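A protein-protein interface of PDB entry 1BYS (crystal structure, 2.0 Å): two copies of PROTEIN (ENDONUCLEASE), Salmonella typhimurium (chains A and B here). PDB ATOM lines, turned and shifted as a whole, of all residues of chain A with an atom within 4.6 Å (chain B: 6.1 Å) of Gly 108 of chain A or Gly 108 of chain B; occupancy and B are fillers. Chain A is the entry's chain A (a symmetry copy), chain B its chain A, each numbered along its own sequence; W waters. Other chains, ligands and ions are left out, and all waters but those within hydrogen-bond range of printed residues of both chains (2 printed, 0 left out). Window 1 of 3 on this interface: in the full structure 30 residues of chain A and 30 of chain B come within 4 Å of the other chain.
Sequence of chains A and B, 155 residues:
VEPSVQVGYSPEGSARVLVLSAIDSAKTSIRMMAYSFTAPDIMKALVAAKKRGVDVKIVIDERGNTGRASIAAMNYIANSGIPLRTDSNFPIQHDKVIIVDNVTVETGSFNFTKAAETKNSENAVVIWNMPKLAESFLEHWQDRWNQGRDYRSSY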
ATOM      1  N   LYS A  96      23.568  -8.272  26.789  1.00  0.00           N
ATOM      2  CA  LYS A  96      24.924  -8.332  27.346  1.00  0.00           C
ATOM      3  C   LYS A  96      24.671  -7.703  28.698  1.00  0.00           C
ATOM      4  O   LYS A  96      24.880  -6.503  28.895  1.00  0.00           O
ATOM      5  CB  LYS A  96      25.903  -7.467  26.559  1.00  0.00           C
ATOM      6  CG  LYS A  96      25.978  -7.789  25.090  1.00  0.00           C
ATOM      7  CD  LYS A  96      25.095  -6.796  24.306  1.00  0.00           C
ATOM      8  CE  LYS A  96      25.391  -6.886  22.823  1.00  0.00           C
ATOM      9  NZ  LYS A  96      24.986  -8.223  22.278  1.00  0.00           N
ATOM     10  N   THR A 107      24.982  -3.230  31.858  1.00  0.00           N
ATOM     11  CA  THR A 107      24.416  -3.454  30.534  1.00  0.00           C
ATOM     12  C   THR A 107      25.122  -2.552  29.537  1.00  0.00           C
ATOM     13  O   THR A 107      26.023  -1.814  29.909  1.00  0.00           O
ATOM     14  CB  THR A 107      22.882  -3.237  30.472  1.00  0.00           C
ATOM     15  OG1 THR A 107      22.406  -3.711  29.196  1.00  0.00           O
ATOM     16  CG2 THR A 107      22.518  -1.752  30.674  1.00  0.00           C
ATOM     17  N   GLY A 108      24.741  -2.623  28.272  1.00  0.00           N
ATOM     18  CA  GLY A 108      25.408  -1.814  27.272  1.00  0.00           C
ATOM     19  C   GLY A 108      25.607  -2.607  25.985  1.00  0.00           C
ATOM     20  O   GLY A 108      24.991  -3.653  25.812  1.00  0.00           O
ATOM     21  N   SER A 109      26.467  -2.109  25.098  1.00  0.00           N
ATOM     22  CA  SER A 109      26.746  -2.768  23.817  1.00  0.00           C
ATOM     23  C   SER A 109      27.814  -3.842  23.952  1.00  0.00           C
ATOM     24  O   SER A 109      27.901  -4.768  23.135  1.00  0.00           O
ATOM     25  CB  SER A 109      27.231  -1.731  22.791  1.00  0.00           C
ATOM     26  OG  SER A 109      28.561  -1.277  23.053  1.00  0.00           O
ATOM     27  N   PHE A 110      28.624  -3.694  24.992  1.00  0.00           N
ATOM     28  CA  PHE A 110      29.748  -4.573  25.306  1.00  0.00           C
ATOM     29  C   PHE A 110      29.496  -6.080  25.402  1.00  0.00           C
ATOM     30  O   PHE A 110      28.894  -6.559  26.368  1.00  0.00           O
ATOM     31  CB  PHE A 110      30.368  -4.058  26.610  1.00  0.00           C
ATOM     32  CG  PHE A 110      31.667  -4.734  27.011  1.00  0.00           C
ATOM     33  CD1 PHE A 110      31.655  -5.863  27.807  1.00  0.00           C
ATOM     34  CD2 PHE A 110      32.885  -4.170  26.680  1.00  0.00           C
ATOM     35  CE1 PHE A 110      32.846  -6.416  28.284  1.00  0.00           C
ATOM     36  CE2 PHE A 110      34.081  -4.711  27.145  1.00  0.00           C
ATOM     37  CZ  PHE A 110      34.059  -5.838  27.953  1.00  0.00           C
ATOM     38  N   ASN A 123      30.364   0.611  24.829  1.00  0.00           N
ATOM     39  CA  ASN A 123      30.061   1.303  26.072  1.00  0.00           C
ATOM     40  C   ASN A 123      29.467   0.267  27.035  1.00  0.00           C
ATOM     41  O   ASN A 123      28.768  -0.673  26.619  1.00  0.00           O
ATOM     42  CB  ASN A 123      29.063   2.450  25.852  1.00  0.00           C
ATOM     43  CG  ASN A 123      27.682   1.962  25.454  1.00  0.00           C
ATOM     44  OD1 ASN A 123      27.444   1.622  24.291  1.00  0.00           O
ATOM     45  ND2 ASN A 123      26.768   1.918  26.409  1.00  0.00           N
ATOM     46  N   ALA A 124      29.786   0.406  28.312  1.00  0.00           N
ATOM     47  CA  ALA A 124      29.246  -0.473  29.333  1.00  0.00           C
ATOM     48  C   ALA A 124      28.874   0.443  30.482  1.00  0.00           C
ATOM     49  O   ALA A 124      29.640   1.357  30.828  1.00  0.00           O
ATOM     50  CB  ALA A 124      30.302  -1.511  29.800  1.00  0.00           C
ATOM     51  N   ASP B  95      28.487   0.644  19.532  1.00  0.00           N
ATOM     52  CA  ASP B  95      27.508   1.315  20.406  1.00  0.00           C
ATOM     53  C   ASP B  95      26.100   1.458  19.817  1.00  0.00           C
ATOM     54  O   ASP B  95      25.948   1.658  18.605  1.00  0.00           O
ATOM     55  CB  ASP B  95      27.993   2.733  20.771  1.00  0.00           C
ATOM     56  CG  ASP B  95      29.454   2.769  21.207  1.00  0.00           C
ATOM     57  OD1 ASP B  95      30.351   2.842  20.331  1.00  0.00           O
ATOM     58  OD2 ASP B  95      29.701   2.732  22.429  1.00  0.00           O
ATOM     59  N   LYS B  96      25.085   1.343  20.673  1.00  0.00           N
ATOM     60  CA  LYS B  96      23.679   1.524  20.294  1.00  0.00           C
ATOM     61  C   LYS B  96      23.260   2.528  21.344  1.00  0.00           C
ATOM     62  O   LYS B  96      22.704   2.171  22.386  1.00  0.00           O
ATOM     63  CB  LYS B  96      22.871   0.242  20.467  1.00  0.00           C
ATOM     64  CG  LYS B  96      23.417  -0.944  19.718  1.00  0.00           C
ATOM     65  CD  LYS B  96      24.249  -1.816  20.682  1.00  0.00           C
ATOM     66  CE  LYS B  96      24.544  -3.162  20.053  1.00  0.00           C
ATOM     67  NZ  LYS B  96      25.436  -3.009  18.857  1.00  0.00           N
ATOM     68  N   VAL B  97      23.529   3.792  21.054  1.00  0.00           N
ATOM     69  CA  VAL B  97      23.303   4.856  22.014  1.00  0.00           C
ATOM     70  C   VAL B  97      22.597   6.093  21.490  1.00  0.00           C
ATOM     71  O   VAL B  97      22.846   6.525  20.362  1.00  0.00           O
ATOM     72  CB  VAL B  97      24.666   5.324  22.560  1.00  0.00           C
ATOM     73  CG1 VAL B  97      24.509   6.640  23.318  1.00  0.00           C
ATOM     74  CG2 VAL B  97      25.283   4.254  23.422  1.00  0.00           C
ATOM     75  N   GLU B 106      20.185   6.844  26.333  1.00  0.00           N
ATOM     76  CA  GLU B 106      19.544   5.577  26.037  1.00  0.00           C
ATOM     77  C   GLU B 106      20.714   4.681  25.625  1.00  0.00           C
ATOM     78  O   GLU B 106      21.625   5.114  24.903  1.00  0.00           O
ATOM     79  CB  GLU B 106      18.548   5.709  24.869  1.00  0.00           C
ATOM     80  CG  GLU B 106      17.801   4.416  24.495  1.00  0.00           C
ATOM     81  CD  GLU B 106      18.625   3.491  23.608  1.00  0.00           C
ATOM     82  OE1 GLU B 106      19.474   3.992  22.839  1.00  0.00           O
ATOM     83  OE2 GLU B 106      18.422   2.257  23.685  1.00  0.00           O
ATOM     84  N   THR B 107      20.729   3.455  26.122  1.00  0.00           N
ATOM     85  CA  THR B 107      21.774   2.515  25.735  1.00  0.00           C
ATOM     86  C   THR B 107      21.279   1.101  25.977  1.00  0.00           C
ATOM     87  O   THR B 107      20.152   0.911  26.413  1.00  0.00           O
ATOM     88  CB  THR B 107      23.121   2.753  26.464  1.00  0.00           C
ATOM     89  OG1 THR B 107      24.129   1.933  25.839  1.00  0.00           O
ATOM     90  CG2 THR B 107      23.008   2.428  27.968  1.00  0.00           C
ATOM     91  N   GLY B 108      22.098   0.106  25.676  1.00  0.00           N
ATOM     92  CA  GLY B 108      21.662  -1.264  25.850  1.00  0.00           C
ATOM     93  C   GLY B 108      22.146  -2.133  24.695  1.00  0.00           C
ATOM     94  O   GLY B 108      23.020  -1.716  23.943  1.00  0.00           O
ATOM     95  N   SER B 109      21.572  -3.327  24.558  1.00  0.00           N
ATOM     96  CA  SER B 109      21.949  -4.264  23.493  1.00  0.00           C
ATOM     97  C   SER B 109      21.205  -3.979  22.197  1.00  0.00           C
ATOM     98  O   SER B 109      21.652  -4.353  21.105  1.00  0.00           O
ATOM     99  CB  SER B 109      21.630  -5.704  23.926  1.00  0.00           C
ATOM    100  OG  SER B 109      20.227  -5.982  23.923  1.00  0.00           O
ATOM    101  N   PHE B 110      20.064  -3.321  22.344  1.00  0.00           N
ATOM    102  CA  PHE B 110      19.157  -2.969  21.254  1.00  0.00           C
ATOM    103  C   PHE B 110      19.721  -2.220  20.043  1.00  0.00           C
ATOM    104  O   PHE B 110      20.030  -1.028  20.127  1.00  0.00           O
ATOM    105  CB  PHE B 110      17.999  -2.177  21.871  1.00  0.00           C
ATOM    106  CG  PHE B 110      16.853  -1.874  20.923  1.00  0.00           C
ATOM    107  CD1 PHE B 110      16.854  -0.717  20.168  1.00  0.00           C
ATOM    108  CD2 PHE B 110      15.740  -2.692  20.880  1.00  0.00           C
ATOM    109  CE1 PHE B 110      15.748  -0.369  19.389  1.00  0.00           C
ATOM    110  CE2 PHE B 110      14.630  -2.361  20.107  1.00  0.00           C
ATOM    111  CZ  PHE B 110      14.635  -1.192  19.361  1.00  0.00           C
ATOM    112  N   ASN B 111      19.865  -2.903  18.912  1.00  0.00           N
ATOM    113  CA  ASN B 111      20.329  -2.227  17.695  1.00  0.00           C
ATOM    114  C   ASN B 111      19.064  -1.594  17.080  1.00  0.00           C
ATOM    115  O   ASN B 111      17.939  -2.050  17.337  1.00  0.00           O
ATOM    116  CB  ASN B 111      20.904  -3.208  16.663  1.00  0.00           C
ATOM    117  CG  ASN B 111      22.359  -3.563  16.923  1.00  0.00           C
ATOM    118  OD1 ASN B 111      22.666  -4.708  17.190  1.00  0.00           O
ATOM    119  ND2 ASN B 111      23.254  -2.593  16.830  1.00  0.00           N
ATOM    120  N   ASN B 123      17.497  -5.614  25.465  1.00  0.00           N
ATOM    121  CA  ASN B 123      17.147  -4.718  26.556  1.00  0.00           C
ATOM    122  C   ASN B 123      17.587  -3.307  26.144  1.00  0.00           C
ATOM    123  O   ASN B 123      18.598  -3.126  25.444  1.00  0.00           O
ATOM    124  CB  ASN B 123      17.840  -5.124  27.865  1.00  0.00           C
ATOM    125  CG  ASN B 123      19.346  -4.939  27.817  1.00  0.00           C
ATOM    126  OD1 ASN B 123      20.066  -5.771  27.256  1.00  0.00           O
ATOM    127  ND2 ASN B 123      19.831  -3.853  28.395  1.00  0.00           N
ATOM    128  N   ALA B 124      16.803  -2.314  26.532  1.00  0.00           N
ATOM    129  CA  ALA B 124      17.134  -0.928  26.255  1.00  0.00           C
ATOM    130  C   ALA B 124      16.825  -0.188  27.541  1.00  0.00           C
ATOM    131  O   ALA B 124      15.786  -0.436  28.173  1.00  0.00           O
ATOM    132  CB  ALA B 124      16.272  -0.362  25.095  1.00  0.00           C
ATOM    133  N   VAL B 125      17.737   0.676  27.961  1.00  0.00           N
ATOM    134  CA  VAL B 125      17.506   1.458  29.156  1.00  0.00           C
ATOM    135  C   VAL B 125      17.605   2.931  28.809  1.00  0.00           C
ATOM    136  O   VAL B 125      18.312   3.325  27.879  1.00  0.00           O
ATOM    137  CB  VAL B 125      18.542   1.150  30.278  1.00  0.00           C
ATOM    138  CG1 VAL B 125      18.258  -0.203  30.881  1.00  0.00           C
ATOM    139  CG2 VAL B 125      19.960   1.220  29.725  1.00  0.00           C
HETATM  140  O   HOH W   1      25.027   0.441  23.302  1.00  0.00           O
HETATM  141  O   HOH W   2      22.888  -5.576  26.796  1.00  0.00           O
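OD2 of Asp 95 of chain B sits close to OD1 of Asn 123 of chain A, 3.1 Å away. The side-chain hydroxyl (OG1) of Thr 107 of chain B sits at hydrogen-bond distance from the side-chain amide nitrogen (ND2) of Asn 123 of chain A. The side-chain hydroxyl of Thr 107 of chain A is in hydrogen-bond range of the side-chain amide nitrogen of Asn 123 of chain B (2.7 Å). O of Gly 108 of chain B sits close to O of Gly 108 of chain A.
NZ of Lys 96 of chain B lies close to ND2 of Asn 111 of chain B, at 3.0 Å. The backbone carbonyl oxygen (O) of Thr 107 of chain B lies within hydrogen-bond range of the backbone NH (N) of Val 125 of chain B. The backbone NH (N) of Ser 109 of chain B is in hydrogen-bond range of the backbone carbonyl oxygen (O) of Asn 123 of chain B, 3.1 Å away. The backbone NH (N) of Phe 110 of chain B sits at hydrogen-bond distance from the backbone carbonyl oxygen (O) of Asn 123 of chain B. O of Asn 123 of chain A sits at hydrogen-bond distance from N of Ser 109 of chain A. N of Phe 110 of chain A sits at hydrogen-bond distance from O of Asn 123 of chain A, 3.4 Å away.
Among the printed residues, merely in contact across the chains: Lys 96 of chain A with Ser 109 of chain B (3.7 Å), Gly 108 of chain A with Ser 109 of chain B (3.7 Å), Ser 109 of chain A with Asp 95 of chain B (3.9 Å), Ser 109 of chain A with Lys 96 of chain B (3.7 Å), Ser 109 of chain A with Gly 108 of chain B (3.7 Å) and Asn 123 of chain A with Val 97 of chain B (3.5 Å).
Of the printed residues of chain B, Thr 107 of chain A touches Asn 123. Printed residues of chain A within 4 Å of Asp 95 of chain B: Ser 109 (3.9 Å) and Asn 123 (3.1 Å). Printed residues of chain A within 4 Å of Val 97 of chain B: Asn 123 (3.5 Å). Gly 108 of chain B touches two residues of chain A. Phe 110 of chain B touches none of the printed residues of chain A. Val 125 of chain B touches none of the printed residues of chain A. The nearest residue of chain B that does not touch Gly 108 of chain A is Thr 107 of chain B (4.2 Å). The nearest residue of chain A that does not touch Gly 108 of chain B is Thr 107 of chain A (4.2 Å). The nearest printed residue of chain A that does not touch Asp 95 of chain B is Ala 124 of chain A (6.3 Å).
Of the 7 printed residues of chain A, 5 touch a printed residue of chain B. Among the printed residues, 10 pairs touch across the chains. Among the printed residues, no Asp or Glu carboxylate lies within 4 Å of a Lys or Arg side-chain nitrogen of the other chain.
Lys 96 of chain A touches Ser 109 of chain B, and with the chains exchanged Ser 109 of chain A touches Lys 96 of chain B. Thr 107 of chain A touches Asn 123 of chain B, and with the chains exchanged Asn 123 of chain A touches Thr 107 of chain B. Gly 108 of chain B touches its own counterpart, Gly 108 of chain A. Gly 108 of chain A touches Ser 109 of chain B, and with the chains exchanged Ser 109 of chain A touches Gly 108 of chain B.
Water W1 lies within hydrogen-bond range of N of Lys 96 of chain B (2.8 Å), OD1 of Asn 123 of chain A (2.9 Å), O of Gly 108 of chain B (3.0 Å), OG1 of Thr 107 of chain B (3.1 Å) and N of Ser 109 of chain A (3.4 Å). Water W2 lies within hydrogen-bond range of the backbone NH of Lys 96 of chain A, the side-chain amide oxygen of Asn 123 of chain B, the backbone carbonyl oxygen of Gly 108 of chain A, the side-chain hydroxyl of Thr 107 of chain A and the backbone NH of Ser 109 of chain B.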
